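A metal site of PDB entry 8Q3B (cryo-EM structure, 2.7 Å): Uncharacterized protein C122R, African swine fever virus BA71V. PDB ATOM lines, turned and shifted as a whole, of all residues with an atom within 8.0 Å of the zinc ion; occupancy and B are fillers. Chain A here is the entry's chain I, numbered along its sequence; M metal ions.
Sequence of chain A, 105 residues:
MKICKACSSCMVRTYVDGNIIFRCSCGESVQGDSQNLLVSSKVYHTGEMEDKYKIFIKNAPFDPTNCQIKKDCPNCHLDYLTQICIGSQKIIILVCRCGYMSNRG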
ATOM      1  N   ILE A   3     -18.964 -33.423 -30.785  1.00  0.00           N
ATOM      2  CA  ILE A   3     -20.254 -33.717 -31.405  1.00  0.00           C
ATOM      3  C   ILE A   3     -21.334 -33.558 -30.348  1.00  0.00           C
ATOM      4  O   ILE A   3     -21.268 -34.191 -29.291  1.00  0.00           O
ATOM      5  CB  ILE A   3     -20.269 -35.138 -32.014  1.00  0.00           C
ATOM      6  CG1 ILE A   3     -19.446 -35.188 -33.305  1.00  0.00           C
ATOM      7  CG2 ILE A   3     -21.695 -35.580 -32.272  1.00  0.00           C
ATOM      8  CD1 ILE A   3     -19.930 -34.244 -34.405  1.00  0.00           C
ATOM      9  N   CYS A   4     -22.324 -32.724 -30.642  1.00  0.00           N
ATOM     10  CA  CYS A   4     -23.424 -32.515 -29.704  1.00  0.00           C
ATOM     11  C   CYS A   4     -24.165 -33.829 -29.491  1.00  0.00           C
ATOM     12  O   CYS A   4     -24.327 -34.626 -30.404  1.00  0.00           O
ATOM     13  CB  CYS A   4     -24.360 -31.427 -30.248  1.00  0.00           C
ATOM     14  SG  CYS A   4     -25.652 -30.853 -29.114  1.00  0.00           S
ATOM     15  N   LYS A   5     -24.580 -34.059 -28.245  1.00  0.00           N
ATOM     16  CA  LYS A   5     -25.269 -35.309 -27.926  1.00  0.00           C
ATOM     17  C   LYS A   5     -26.663 -35.345 -28.560  1.00  0.00           C
ATOM     18  O   LYS A   5     -27.065 -36.356 -29.137  1.00  0.00           O
ATOM     19  CB  LYS A   5     -25.372 -35.495 -26.411  1.00  0.00           C
ATOM     20  CG  LYS A   5     -24.057 -35.327 -25.619  1.00  0.00           C
ATOM     21  CD  LYS A   5     -22.749 -35.781 -26.290  1.00  0.00           C
ATOM     22  CE  LYS A   5     -22.809 -37.142 -27.009  1.00  0.00           C
ATOM     23  NZ  LYS A   5     -23.652 -38.155 -26.301  1.00  0.00           N
ATOM     24  N   ALA A   6     -27.403 -34.238 -28.458  1.00  0.00           N
ATOM     25  CA  ALA A   6     -28.754 -34.203 -29.019  1.00  0.00           C
ATOM     26  C   ALA A   6     -28.720 -34.337 -30.539  1.00  0.00           C
ATOM     27  O   ALA A   6     -29.521 -35.086 -31.117  1.00  0.00           O
ATOM     28  CB  ALA A   6     -29.448 -32.904 -28.618  1.00  0.00           C
ATOM     29  N   CYS A   7     -27.808 -33.624 -31.195  1.00  0.00           N
ATOM     30  CA  CYS A   7     -27.657 -33.664 -32.639  1.00  0.00           C
ATOM     31  C   CYS A   7     -26.201 -33.920 -32.971  1.00  0.00           C
ATOM     32  O   CYS A   7     -25.309 -33.463 -32.260  1.00  0.00           O
ATOM     33  CB  CYS A   7     -28.102 -32.349 -33.281  1.00  0.00           C
ATOM     34  SG  CYS A   7     -27.266 -30.888 -32.606  1.00  0.00           S
ATOM     35  N   SER A   8     -25.947 -34.654 -34.044  1.00  0.00           N
ATOM     36  CA  SER A   8     -24.569 -34.947 -34.423  1.00  0.00           C
ATOM     37  C   SER A   8     -23.964 -33.775 -35.174  1.00  0.00           C
ATOM     38  O   SER A   8     -23.546 -33.926 -36.327  1.00  0.00           O
ATOM     39  CB  SER A   8     -24.505 -36.228 -35.246  1.00  0.00           C
ATOM     40  OG  SER A   8     -24.900 -37.353 -34.489  1.00  0.00           O
ATOM     41  N   SER A   9     -23.905 -32.616 -34.536  1.00  0.00           N
ATOM     42  CA  SER A   9     -23.365 -31.396 -35.129  1.00  0.00           C
ATOM     43  C   SER A   9     -22.125 -30.940 -34.372  1.00  0.00           C
ATOM     44  O   SER A   9     -21.968 -31.225 -33.178  1.00  0.00           O
ATOM     45  CB  SER A   9     -24.405 -30.277 -35.138  1.00  0.00           C
ATOM     46  OG  SER A   9     -23.794 -29.015 -34.987  1.00  0.00           O
ATOM     47  N   CYS A  10     -21.259 -30.223 -35.075  1.00  0.00           N
ATOM     48  CA  CYS A  10     -20.022 -29.734 -34.481  1.00  0.00           C
ATOM     49  C   CYS A  10     -20.302 -28.601 -33.497  1.00  0.00           C
ATOM     50  O   CYS A  10     -21.198 -27.788 -33.698  1.00  0.00           O
ATOM     51  CB  CYS A  10     -19.058 -29.262 -35.565  1.00  0.00           C
ATOM     52  SG  CYS A  10     -18.840 -30.413 -36.934  1.00  0.00           S
ATOM     53  N   MET A  11     -19.499 -28.561 -32.427  1.00  0.00           N
ATOM     54  CA  MET A  11     -19.559 -27.513 -31.419  1.00  0.00           C
ATOM     55  C   MET A  11     -18.378 -26.559 -31.585  1.00  0.00           C
ATOM     56  O   MET A  11     -17.240 -27.003 -31.798  1.00  0.00           O
ATOM     57  CB  MET A  11     -19.536 -28.105 -30.011  1.00  0.00           C
ATOM     58  CG  MET A  11     -20.131 -29.500 -29.887  1.00  0.00           C
ATOM     59  SD  MET A  11     -20.681 -29.821 -28.203  1.00  0.00           S
ATOM     60  CE  MET A  11     -22.372 -29.242 -28.214  1.00  0.00           C
ATOM     61  N   PHE A  22     -18.231 -25.844 -25.134  1.00  0.00           N
ATOM     62  CA  PHE A  22     -18.568 -26.238 -26.495  1.00  0.00           C
ATOM     63  C   PHE A  22     -20.004 -25.812 -26.781  1.00  0.00           C
ATOM     64  O   PHE A  22     -20.951 -26.446 -26.322  1.00  0.00           O
ATOM     65  CB  PHE A  22     -18.389 -27.740 -26.685  1.00  0.00           C
ATOM     66  CG  PHE A  22     -16.962 -28.193 -26.564  1.00  0.00           C
ATOM     67  CD1 PHE A  22     -16.075 -28.015 -27.611  1.00  0.00           C
ATOM     68  CD2 PHE A  22     -16.506 -28.803 -25.408  1.00  0.00           C
ATOM     69  CE1 PHE A  22     -14.771 -28.444 -27.508  1.00  0.00           C
ATOM     70  CE2 PHE A  22     -15.206 -29.227 -25.297  1.00  0.00           C
ATOM     71  CZ  PHE A  22     -14.327 -29.049 -26.348  1.00  0.00           C
ATOM     72  N   ARG A  23     -20.170 -24.746 -27.558  1.00  0.00           N
ATOM     73  CA  ARG A  23     -21.483 -24.245 -27.919  1.00  0.00           C
ATOM     74  C   ARG A  23     -21.963 -24.882 -29.216  1.00  0.00           C
ATOM     75  O   ARG A  23     -21.177 -25.184 -30.111  1.00  0.00           O
ATOM     76  CB  ARG A  23     -21.454 -22.714 -28.070  1.00  0.00           C
ATOM     77  CG  ARG A  23     -22.796 -22.103 -28.453  1.00  0.00           C
ATOM     78  CD  ARG A  23     -23.184 -20.950 -27.528  1.00  0.00           C
ATOM     79  NE  ARG A  23     -23.563 -21.401 -26.208  1.00  0.00           N
ATOM     80  CZ  ARG A  23     -22.800 -21.333 -25.123  1.00  0.00           C
ATOM     81  NH1 ARG A  23     -21.582 -20.806 -25.164  1.00  0.00           N
ATOM     82  NH2 ARG A  23     -23.268 -21.779 -23.959  1.00  0.00           N
ATOM     83  N   CYS A  24     -23.286 -25.076 -29.303  1.00  0.00           N
ATOM     84  CA  CYS A  24     -23.927 -25.643 -30.474  1.00  0.00           C
ATOM     85  C   CYS A  24     -25.039 -24.719 -30.932  1.00  0.00           C
ATOM     86  O   CYS A  24     -25.506 -23.853 -30.180  1.00  0.00           O
ATOM     87  CB  CYS A  24     -24.491 -27.038 -30.182  1.00  0.00           C
ATOM     88  SG  CYS A  24     -25.049 -27.960 -31.628  1.00  0.00           S
ATOM     89  N   SER A  25     -25.464 -24.900 -32.181  1.00  0.00           N
ATOM     90  CA  SER A  25     -26.553 -24.082 -32.711  1.00  0.00           C
ATOM     91  C   SER A  25     -27.842 -24.272 -31.929  1.00  0.00           C
ATOM     92  O   SER A  25     -28.687 -23.365 -31.917  1.00  0.00           O
ATOM     93  CB  SER A  25     -26.794 -24.412 -34.191  1.00  0.00           C
ATOM     94  OG  SER A  25     -26.597 -25.798 -34.438  1.00  0.00           O
ATOM     95  N   CYS A  26     -28.020 -25.421 -31.281  1.00  0.00           N
ATOM     96  CA  CYS A  26     -29.203 -25.703 -30.482  1.00  0.00           C
ATOM     97  C   CYS A  26     -28.971 -25.440 -28.999  1.00  0.00           C
ATOM     98  O   CYS A  26     -29.869 -25.688 -28.191  1.00  0.00           O
ATOM     99  CB  CYS A  26     -29.647 -27.152 -30.679  1.00  0.00           C
ATOM    100  SG  CYS A  26     -28.437 -28.378 -30.103  1.00  0.00           S
ATOM    101  N   GLY A  27     -27.799 -24.938 -28.621  1.00  0.00           N
ATOM    102  CA  GLY A  27     -27.454 -24.805 -27.220  1.00  0.00           C
ATOM    103  C   GLY A  27     -26.651 -26.001 -26.762  1.00  0.00           C
ATOM    104  O   GLY A  27     -25.592 -26.301 -27.311  1.00  0.00           O
ATOM    105  N   GLU A  28     -27.154 -26.694 -25.728  1.00  0.00           N
ATOM    106  CA  GLU A  28     -26.546 -27.932 -25.260  1.00  0.00           C
ATOM    107  C   GLU A  28     -25.047 -27.760 -25.019  1.00  0.00           C
ATOM    108  O   GLU A  28     -24.236 -28.586 -25.420  1.00  0.00           O
ATOM    109  CB  GLU A  28     -26.815 -29.078 -26.240  1.00  0.00           C
ATOM    110  CG  GLU A  28     -28.215 -29.679 -26.162  1.00  0.00           C
ATOM    111  CD  GLU A  28     -29.330 -28.654 -26.215  1.00  0.00           C
ATOM    112  OE1 GLU A  28     -30.494 -29.025 -25.975  1.00  0.00           O
ATOM    113  OE2 GLU A  28     -29.046 -27.469 -26.511  1.00  0.00           O
ATOM    114  N   SER A  29     -24.685 -26.663 -24.351  1.00  0.00           N
ATOM    115  CA  SER A  29     -23.274 -26.385 -24.116  1.00  0.00           C
ATOM    116  C   SER A  29     -22.660 -27.453 -23.223  1.00  0.00           C
ATOM    117  O   SER A  29     -23.333 -28.045 -22.368  1.00  0.00           O
ATOM    118  CB  SER A  29     -23.107 -25.001 -23.481  1.00  0.00           C
ATOM    119  OG  SER A  29     -23.703 -24.959 -22.191  1.00  0.00           O
HETATM  120 ZN    ZN M   1     -26.557 -29.548 -30.828  1.00  0.00          ZN
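The side-chain carboxylate (OE2) of Glu 28 sits close to the side-chain sulfur (SG) of Cys 26. SG of Cys 24 lies close to OG of Ser 9. The backbone NH (N) of Cys 4 lies within hydrogen-bond range of the backbone carbonyl oxygen (O) of Ser 9, at 3.0 Å.
Of the 17 residues printed, 4 come within 4 Å of the zinc ion.
The zinc ion is bound by SG of Cys 26 (2.3 Å), SG of Cys 24 (2.3 Å), SG of Cys 7 (2.3 Å) and SG of Cys 4 (2.3 Å).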
